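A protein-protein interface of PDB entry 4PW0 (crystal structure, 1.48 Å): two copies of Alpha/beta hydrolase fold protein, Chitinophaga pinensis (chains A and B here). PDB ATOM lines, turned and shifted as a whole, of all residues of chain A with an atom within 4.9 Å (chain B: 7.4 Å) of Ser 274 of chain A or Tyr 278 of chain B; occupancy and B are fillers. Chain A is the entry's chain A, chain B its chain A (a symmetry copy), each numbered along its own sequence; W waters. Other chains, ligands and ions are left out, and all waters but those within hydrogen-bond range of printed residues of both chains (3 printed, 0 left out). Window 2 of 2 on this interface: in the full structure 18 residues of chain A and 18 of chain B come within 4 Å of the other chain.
N of Leu 271 of chain A is in hydrogen-bond range of OH of Tyr 278 of chain B, at 3.5 Å.
N of Tyr 283 of chain B sits at hydrogen-bond distance from O of Tyr 278 of chain B.
CB of Glu 270 of chain A touches OH of Tyr 278 of chain B, at 3.4 Å.
CD1 of Ile 253 of chain B touches CD2 of Leu 271 of chain A, 3.9 Å away.
Tyr 278 of chain B touches Ser 274 of chain A.
Tyr 278 of chain A touches Ser 274 of chain B (CD1 to OG, 3.4 Å).
Of chain B, only Tyr 278 (3.4 Å) comes within 4 Å of Ser 274 of chain A.
Printed residues of chain A within 4 Å of Tyr 278 of chain B: Glu 270 (3.4 Å), Leu 271 (3.5 Å) and Ser 274 (3.4 Å).
Printed residues of chain B within 4 Å of Tyr 278 of chain A: Ser 274 (3.4 Å).
Of the printed residues of chain A, Ile 253 of chain B touches Leu 271 (3.9 Å).
Of the printed residues of chain B, Glu 270 of chain A touches Tyr 278 (3.4 Å).
Printed residues of chain A that touch a printed residue of chain B: Glu 270, Leu 271, Ser 274 and Tyr 278.
Hydrophobic or aromatic side chains of chain A that line the printed part of chain B: Leu 271 and Tyr 278.
Along chain A the printed residues that touch a printed residue of chain B span positions 270 to 278.
Among the printed residues, no Asp or Glu carboxylate lies within 4 Å of a Lys or Arg side-chain nitrogen of the other chain.
Ser 274 of chain A touches Tyr 278 of chain B, and with the chains exchanged Tyr 278 of chain A touches Ser 274 of chain B.
Water W2 lies within hydrogen-bond range of OE1 of Glu 270 of chain A (2.5 Å) and OH of Tyr 278 of chain B (2.7 Å).
Water W1 lies within hydrogen-bond range of OG of Ser 274 of chain B (2.7 Å) and O of Ser 274 of chain A (3.4 Å).
Water W3 lies within hydrogen-bond range of the side-chain hydroxyl of Ser 274 of chain A (2.7 Å) and the backbone carbonyl oxygen of Ser 274 of chain B (3.4 Å).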
ATOM      1  N   GLU A 270      -9.044   3.757 -28.922  1.00  0.00           N
ATOM      2  CA  GLU A 270      -8.772   4.926 -28.106  1.00  0.00           C
ATOM      3  C   GLU A 270      -7.745   5.890 -28.740  1.00  0.00           C
ATOM      4  O   GLU A 270      -7.864   7.123 -28.650  1.00  0.00           O
ATOM      5  CB  GLU A 270      -8.367   4.512 -26.701  1.00  0.00           C
ATOM      6  CG  GLU A 270      -9.531   3.869 -25.973  1.00  0.00           C
ATOM      7  CD  GLU A 270      -9.345   3.767 -24.487  1.00  0.00           C
ATOM      8  OE1 GLU A 270      -8.227   3.464 -24.032  1.00  0.00           O
ATOM      9  OE2 GLU A 270     -10.352   3.980 -23.788  1.00  0.00           O
ATOM     10  N   LEU A 271      -6.773   5.309 -29.456  1.00  0.00           N
ATOM     11  CA  LEU A 271      -5.837   6.115 -30.229  1.00  0.00           C
ATOM     12  C   LEU A 271      -6.629   6.897 -31.313  1.00  0.00           C
ATOM     13  O   LEU A 271      -6.440   8.097 -31.516  1.00  0.00           O
ATOM     14  CB  LEU A 271      -4.804   5.217 -30.872  1.00  0.00           C
ATOM     15  CG  LEU A 271      -3.807   5.823 -31.837  1.00  0.00           C
ATOM     16  CD1 LEU A 271      -2.979   6.916 -31.202  1.00  0.00           C
ATOM     17  CD2 LEU A 271      -2.912   4.725 -32.437  1.00  0.00           C
ATOM     18  N   PHE A 272      -7.491   6.162 -32.011  1.00  0.00           N
ATOM     19  CA  PHE A 272      -8.306   6.799 -33.059  1.00  0.00           C
ATOM     20  C   PHE A 272      -9.145   7.949 -32.509  1.00  0.00           C
ATOM     21  O   PHE A 272      -9.201   9.017 -33.103  1.00  0.00           O
ATOM     22  CB  PHE A 272      -9.191   5.760 -33.744  1.00  0.00           C
ATOM     23  CG  PHE A 272     -10.091   6.352 -34.783  1.00  0.00           C
ATOM     24  CD1 PHE A 272      -9.596   6.693 -36.018  1.00  0.00           C
ATOM     25  CD2 PHE A 272     -11.423   6.613 -34.509  1.00  0.00           C
ATOM     26  CE1 PHE A 272     -10.406   7.256 -36.980  1.00  0.00           C
ATOM     27  CE2 PHE A 272     -12.233   7.200 -35.471  1.00  0.00           C
ATOM     28  CZ  PHE A 272     -11.741   7.524 -36.708  1.00  0.00           C
ATOM     29  N   VAL A 273      -9.840   7.695 -31.394  1.00  0.00           N
ATOM     30  CA  VAL A 273     -10.660   8.764 -30.795  1.00  0.00           C
ATOM     31  C   VAL A 273      -9.806   9.960 -30.418  1.00  0.00           C
ATOM     32  O   VAL A 273     -10.161  11.108 -30.693  1.00  0.00           O
ATOM     33  CB  VAL A 273     -11.445   8.237 -29.593  1.00  0.00           C
ATOM     34  CG1 VAL A 273     -12.060   9.386 -28.815  1.00  0.00           C
ATOM     35  CG2 VAL A 273     -12.507   7.254 -30.040  1.00  0.00           C
ATOM     36  N   SER A 274      -8.651   9.707 -29.785  1.00  0.00           N
ATOM     37  CA  SER A 274      -7.782  10.811 -29.379  1.00  0.00           C
ATOM     38  C   SER A 274      -7.346  11.679 -30.555  1.00  0.00           C
ATOM     39  O   SER A 274      -7.416  12.923 -30.536  1.00  0.00           O
ATOM     40  CB  SER A 274      -6.579  10.283 -28.656  1.00  0.00           C
ATOM     41  OG  SER A 274      -5.710  11.356 -28.307  1.00  0.00           O
ATOM     42  N   GLN A 275      -6.955  10.995 -31.616  1.00  0.00           N
ATOM     43  CA  GLN A 275      -6.506  11.723 -32.811  1.00  0.00           C
ATOM     44  C   GLN A 275      -7.627  12.471 -33.503  1.00  0.00           C
ATOM     45  O   GLN A 275      -7.439  13.645 -33.924  1.00  0.00           O
ATOM     46  CB  GLN A 275      -5.837  10.759 -33.778  1.00  0.00           C
ATOM     47  CG  GLN A 275      -4.550  10.212 -33.260  1.00  0.00           C
ATOM     48  CD  GLN A 275      -3.797   9.443 -34.313  1.00  0.00           C
ATOM     49  OE1 GLN A 275      -4.371   8.900 -35.225  1.00  0.00           O
ATOM     50  NE2 GLN A 275      -2.455   9.373 -34.117  1.00  0.00           N
ATOM     51  N   THR A 276      -8.774  11.796 -33.647  1.00  0.00           N
ATOM     52  CA  THR A 276      -9.940  12.330 -34.356  1.00  0.00           C
ATOM     53  C   THR A 276     -10.594  13.493 -33.604  1.00  0.00           C
ATOM     54  O   THR A 276     -11.022  14.488 -34.215  1.00  0.00           O
ATOM     55  CB  THR A 276     -10.987  11.200 -34.614  1.00  0.00           C
ATOM     56  OG1 THR A 276     -10.376  10.186 -35.395  1.00  0.00           O
ATOM     57  CG2 THR A 276     -12.173  11.727 -35.389  1.00  0.00           C
ATOM     58  N   GLU A 277     -10.656  13.373 -32.275  1.00  0.00           N
ATOM     59  CA  GLU A 277     -11.221  14.441 -31.481  1.00  0.00           C
ATOM     60  C   GLU A 277     -10.405  15.721 -31.634  1.00  0.00           C
ATOM     61  O   GLU A 277     -10.981  16.817 -31.804  1.00  0.00           O
ATOM     62  CB  GLU A 277     -11.302  13.970 -30.021  1.00  0.00           C
ATOM     63  CG  GLU A 277     -11.727  14.972 -29.018  1.00  0.00           C
ATOM     64  CD  GLU A 277     -11.785  14.237 -27.692  1.00  0.00           C
ATOM     65  OE1 GLU A 277     -10.757  13.603 -27.310  1.00  0.00           O
ATOM     66  OE2 GLU A 277     -12.867  14.221 -27.090  1.00  0.00           O
ATOM     67  N   TYR A 278      -9.072  15.642 -31.592  1.00  0.00           N
ATOM     68  CA  TYR A 278      -8.276  16.792 -31.843  1.00  0.00           C
ATOM     69  C   TYR A 278      -8.510  17.378 -33.236  1.00  0.00           C
ATOM     70  O   TYR A 278      -8.660  18.604 -33.440  1.00  0.00           O
ATOM     71  CB  TYR A 278      -6.757  16.538 -31.603  1.00  0.00           C
ATOM     72  CG  TYR A 278      -5.952  17.775 -31.840  1.00  0.00           C
ATOM     73  CD1 TYR A 278      -5.785  18.729 -30.816  1.00  0.00           C
ATOM     74  CD2 TYR A 278      -5.455  18.083 -33.087  1.00  0.00           C
ATOM     75  CE1 TYR A 278      -5.119  19.894 -31.086  1.00  0.00           C
ATOM     76  CE2 TYR A 278      -4.820  19.286 -33.358  1.00  0.00           C
ATOM     77  CZ  TYR A 278      -4.655  20.184 -32.321  1.00  0.00           C
ATOM     78  OH  TYR A 278      -4.056  21.404 -32.600  1.00  0.00           O
ATOM     79  N   LEU B  60       4.361  19.520 -23.677  1.00  0.00           N
ATOM     80  CA  LEU B  60       4.696  18.208 -23.211  1.00  0.00           C
ATOM     81  C   LEU B  60       5.096  18.191 -21.725  1.00  0.00           C
ATOM     82  O   LEU B  60       4.902  17.170 -21.076  1.00  0.00           O
ATOM     83  CB  LEU B  60       5.798  17.580 -24.076  1.00  0.00           C
ATOM     84  CG  LEU B  60       5.272  17.168 -25.466  1.00  0.00           C
ATOM     85  CD1 LEU B  60       6.467  16.715 -26.309  1.00  0.00           C
ATOM     86  CD2 LEU B  60       4.205  16.105 -25.368  1.00  0.00           C
ATOM     87  N   ARG B  64       4.692  15.672 -17.744  1.00  0.00           N
ATOM     88  CA  ARG B  64       5.902  14.948 -17.379  1.00  0.00           C
ATOM     89  C   ARG B  64       7.036  15.935 -17.239  1.00  0.00           C
ATOM     90  O   ARG B  64       6.996  17.051 -17.763  1.00  0.00           O
ATOM     91  CB  ARG B  64       6.273  13.886 -18.436  1.00  0.00           C
ATOM     92  CG  ARG B  64       6.783  14.480 -19.750  1.00  0.00           C
ATOM     93  CD  ARG B  64       6.142  13.864 -20.971  1.00  0.00           C
ATOM     94  NE  ARG B  64       4.779  14.292 -21.148  1.00  0.00           N
ATOM     95  CZ  ARG B  64       3.694  13.509 -21.022  1.00  0.00           C
ATOM     96  NH1 ARG B  64       3.828  12.222 -20.763  1.00  0.00           N
ATOM     97  NH2 ARG B  64       2.495  14.034 -21.154  1.00  0.00           N
ATOM     98  N   LYS B 129       9.551   4.715 -24.218  1.00  0.00           N
ATOM     99  CA  LYS B 129       8.956   5.029 -25.530  1.00  0.00           C
ATOM    100  C   LYS B 129       9.851   6.015 -26.269  1.00  0.00           C
ATOM    101  O   LYS B 129      10.608   6.782 -25.664  1.00  0.00           O
ATOM    102  CB  LYS B 129       7.575   5.661 -25.341  1.00  0.00           C
ATOM    103  CG  LYS B 129       6.577   4.723 -24.639  1.00  0.00           C
ATOM    104  CD  LYS B 129       5.181   5.326 -24.552  1.00  0.00           C
ATOM    105  CE  LYS B 129       4.246   4.524 -23.727  1.00  0.00           C
ATOM    106  NZ  LYS B 129       2.875   5.002 -23.601  1.00  0.00           N
ATOM    107  N   ILE B 253       3.877   3.998 -34.656  1.00  0.00           N
ATOM    108  CA  ILE B 253       2.788   4.786 -35.235  1.00  0.00           C
ATOM    109  C   ILE B 253       3.434   5.868 -36.116  1.00  0.00           C
ATOM    110  O   ILE B 253       4.418   6.486 -35.718  1.00  0.00           O
ATOM    111  CB  ILE B 253       1.957   5.476 -34.126  1.00  0.00           C
ATOM    112  CG1 ILE B 253       1.301   4.487 -33.191  1.00  0.00           C
ATOM    113  CG2 ILE B 253       0.971   6.464 -34.713  1.00  0.00           C
ATOM    114  CD1 ILE B 253       0.960   5.058 -31.830  1.00  0.00           C
ATOM    115  N   PHE B 272       1.174  18.288 -32.898  1.00  0.00           N
ATOM    116  CA  PHE B 272       2.253  17.421 -32.394  1.00  0.00           C
ATOM    117  C   PHE B 272       2.102  17.129 -30.905  1.00  0.00           C
ATOM    118  O   PHE B 272       2.239  15.990 -30.477  1.00  0.00           O
ATOM    119  CB  PHE B 272       3.614  18.049 -32.689  1.00  0.00           C
ATOM    120  CG  PHE B 272       4.757  17.247 -32.150  1.00  0.00           C
ATOM    121  CD1 PHE B 272       5.178  16.113 -32.801  1.00  0.00           C
ATOM    122  CD2 PHE B 272       5.380  17.599 -30.965  1.00  0.00           C
ATOM    123  CE1 PHE B 272       6.217  15.352 -32.310  1.00  0.00           C
ATOM    124  CE2 PHE B 272       6.412  16.820 -30.459  1.00  0.00           C
ATOM    125  CZ  PHE B 272       6.842  15.699 -31.120  1.00  0.00           C
ATOM    126  N   VAL B 273       1.872  18.183 -30.114  1.00  0.00           N
ATOM    127  CA  VAL B 273       1.697  17.975 -28.664  1.00  0.00           C
ATOM    128  C   VAL B 273       0.523  17.056 -28.383  1.00  0.00           C
ATOM    129  O   VAL B 273       0.617  16.133 -27.571  1.00  0.00           O
ATOM    130  CB  VAL B 273       1.545  19.313 -27.938  1.00  0.00           C
ATOM    131  CG1 VAL B 273       1.088  19.091 -26.507  1.00  0.00           C
ATOM    132  CG2 VAL B 273       2.844  20.090 -27.979  1.00  0.00           C
ATOM    133  N   SER B 274      -0.609  17.288 -29.065  1.00  0.00           N
ATOM    134  CA  SER B 274      -1.785  16.450 -28.836  1.00  0.00           C
ATOM    135  C   SER B 274      -1.518  14.974 -29.109  1.00  0.00           C
ATOM    136  O   SER B 274      -1.844  14.072 -28.314  1.00  0.00           O
ATOM    137  CB  SER B 274      -2.932  16.929 -29.677  1.00  0.00           C
ATOM    138  OG  SER B 274      -4.060  16.081 -29.491  1.00  0.00           O
ATOM    139  N   GLN B 275      -0.852  14.742 -30.226  1.00  0.00           N
ATOM    140  CA  GLN B 275      -0.539  13.356 -30.600  1.00  0.00           C
ATOM    141  C   GLN B 275       0.468  12.707 -29.672  1.00  0.00           C
ATOM    142  O   GLN B 275       0.292  11.522 -29.278  1.00  0.00           O
ATOM    143  CB  GLN B 275      -0.041  13.310 -32.036  1.00  0.00           C
ATOM    144  CG  GLN B 275      -1.096  13.657 -33.030  1.00  0.00           C
ATOM    145  CD  GLN B 275      -0.651  13.390 -34.444  1.00  0.00           C
ATOM    146  OE1 GLN B 275       0.515  13.420 -34.752  1.00  0.00           O
ATOM    147  NE2 GLN B 275      -1.660  13.171 -35.327  1.00  0.00           N
ATOM    148  N   THR B 276       1.526  13.458 -29.344  1.00  0.00           N
ATOM    149  CA  THR B 276       2.635  12.974 -28.520  1.00  0.00           C
ATOM    150  C   THR B 276       2.218  12.738 -27.065  1.00  0.00           C
ATOM    151  O   THR B 276       2.636  11.751 -26.433  1.00  0.00           O
ATOM    152  CB  THR B 276       3.837  13.970 -28.580  1.00  0.00           C
ATOM    153  OG1 THR B 276       4.259  14.089 -29.928  1.00  0.00           O
ATOM    154  CG2 THR B 276       5.007  13.456 -27.773  1.00  0.00           C
ATOM    155  N   GLU B 277       1.380  13.636 -26.541  1.00  0.00           N
ATOM    156  CA  GLU B 277       0.902  13.472 -25.186  1.00  0.00           C
ATOM    157  C   GLU B 277       0.094  12.184 -25.050  1.00  0.00           C
ATOM    158  O   GLU B 277       0.278  11.427 -24.072  1.00  0.00           O
ATOM    159  CB  GLU B 277       0.087  14.717 -24.804  1.00  0.00           C
ATOM    160  CG  GLU B 277      -0.608  14.685 -23.498  1.00  0.00           C
ATOM    161  CD  GLU B 277      -1.269  16.041 -23.344  1.00  0.00           C
ATOM    162  OE1 GLU B 277      -2.034  16.447 -24.268  1.00  0.00           O
ATOM    163  OE2 GLU B 277      -0.958  16.724 -22.359  1.00  0.00           O
ATOM    164  N   TYR B 278      -0.801  11.884 -25.996  1.00  0.00           N
ATOM    165  CA  TYR B 278      -1.490  10.641 -25.964  1.00  0.00           C
ATOM    166  C   TYR B 278      -0.546   9.441 -26.033  1.00  0.00           C
ATOM    167  O   TYR B 278      -0.660   8.444 -25.286  1.00  0.00           O
ATOM    168  CB  TYR B 278      -2.594  10.536 -27.059  1.00  0.00           C
ATOM    169  CG  TYR B 278      -3.324   9.235 -26.976  1.00  0.00           C
ATOM    170  CD1 TYR B 278      -4.415   9.080 -26.097  1.00  0.00           C
ATOM    171  CD2 TYR B 278      -2.887   8.118 -27.653  1.00  0.00           C
ATOM    172  CE1 TYR B 278      -5.010   7.854 -25.974  1.00  0.00           C
ATOM    173  CE2 TYR B 278      -3.471   6.871 -27.487  1.00  0.00           C
ATOM    174  CZ  TYR B 278      -4.553   6.766 -26.634  1.00  0.00           C
ATOM    175  OH  TYR B 278      -5.113   5.512 -26.436  1.00  0.00           O
ATOM    176  N   PHE B 279       0.375   9.500 -26.996  1.00  0.00           N
ATOM    177  CA  PHE B 279       1.319   8.434 -27.164  1.00  0.00           C
ATOM    178  C   PHE B 279       2.055   8.128 -25.849  1.00  0.00           C
ATOM    179  O   PHE B 279       2.120   6.988 -25.438  1.00  0.00           O
ATOM    180  CB  PHE B 279       2.296   8.795 -28.275  1.00  0.00           C
ATOM    181  CG  PHE B 279       3.457   7.842 -28.422  1.00  0.00           C
ATOM    182  CD1 PHE B 279       3.271   6.564 -28.939  1.00  0.00           C
ATOM    183  CD2 PHE B 279       4.730   8.221 -28.062  1.00  0.00           C
ATOM    184  CE1 PHE B 279       4.345   5.693 -29.094  1.00  0.00           C
ATOM    185  CE2 PHE B 279       5.812   7.365 -28.211  1.00  0.00           C
ATOM    186  CZ  PHE B 279       5.606   6.111 -28.724  1.00  0.00           C
ATOM    187  N   LEU B 280       2.597   9.152 -25.223  1.00  0.00           N
ATOM    188  CA  LEU B 280       3.370   8.932 -23.988  1.00  0.00           C
ATOM    189  C   LEU B 280       2.505   8.501 -22.813  1.00  0.00           C
ATOM    190  O   LEU B 280       2.930   7.610 -22.058  1.00  0.00           O
ATOM    191  CB  LEU B 280       4.145  10.172 -23.630  1.00  0.00           C
ATOM    192  CG  LEU B 280       5.245  10.562 -24.611  1.00  0.00           C
ATOM    193  CD1 LEU B 280       5.866  11.860 -24.164  1.00  0.00           C
ATOM    194  CD2 LEU B 280       6.306   9.468 -24.761  1.00  0.00           C
ATOM    195  N   ASP B 281       1.315   9.080 -22.693  1.00  0.00           N
ATOM    196  CA  ASP B 281       0.516   8.787 -21.506  1.00  0.00           C
ATOM    197  C   ASP B 281      -0.272   7.511 -21.625  1.00  0.00           C
ATOM    198  O   ASP B 281      -0.523   6.862 -20.597  1.00  0.00           O
ATOM    199  CB  ASP B 281      -0.360   9.981 -21.156  1.00  0.00           C
ATOM    200  CG  ASP B 281       0.456  11.160 -20.693  1.00  0.00           C
ATOM    201  OD1 ASP B 281       1.609  10.941 -20.261  1.00  0.00           O
ATOM    202  OD2 ASP B 281      -0.037  12.304 -20.769  1.00  0.00           O
ATOM    203  N   SER B 282      -0.620   7.103 -22.859  1.00  0.00           N
ATOM    204  CA  SER B 282      -1.611   6.069 -23.019  1.00  0.00           C
ATOM    205  C   SER B 282      -1.330   4.921 -23.965  1.00  0.00           C
ATOM    206  O   SER B 282      -1.921   3.853 -23.797  1.00  0.00           O
ATOM    207  CB  SER B 282      -2.921   6.742 -23.418  1.00  0.00           C
ATOM    208  OG  SER B 282      -3.430   7.604 -22.417  1.00  0.00           O
ATOM    209  N   TYR B 283      -0.504   5.107 -24.995  1.00  0.00           N
ATOM    210  CA  TYR B 283      -0.356   4.048 -25.972  1.00  0.00           C
ATOM    211  C   TYR B 283       0.381   2.830 -25.404  1.00  0.00           C
ATOM    212  O   TYR B 283       1.459   3.014 -24.781  1.00  0.00           O
ATOM    213  CB  TYR B 283       0.363   4.572 -27.229  1.00  0.00           C
ATOM    214  CG  TYR B 283       0.558   3.485 -28.237  1.00  0.00           C
ATOM    215  CD1 TYR B 283      -0.503   3.000 -28.988  1.00  0.00           C
ATOM    216  CD2 TYR B 283       1.818   2.899 -28.433  1.00  0.00           C
ATOM    217  CE1 TYR B 283      -0.317   1.954 -29.855  1.00  0.00           C
ATOM    218  CE2 TYR B 283       2.007   1.855 -29.312  1.00  0.00           C
ATOM    219  CZ  TYR B 283       0.937   1.366 -30.019  1.00  0.00           C
ATOM    220  OH  TYR B 283       1.058   0.298 -30.882  1.00  0.00           O
ATOM    221  OXT TYR B 283      -0.055   1.663 -25.568  1.00  0.00           O
HETATM  222  O   HOH W   1      -4.315  14.086 -31.345  1.00  0.00           O
HETATM  223  O   HOH W   2      -6.119   4.786 -23.983  1.00  0.00           O
HETATM  224  O   HOH W   3      -3.689  11.823 -30.090  1.00  0.00           O
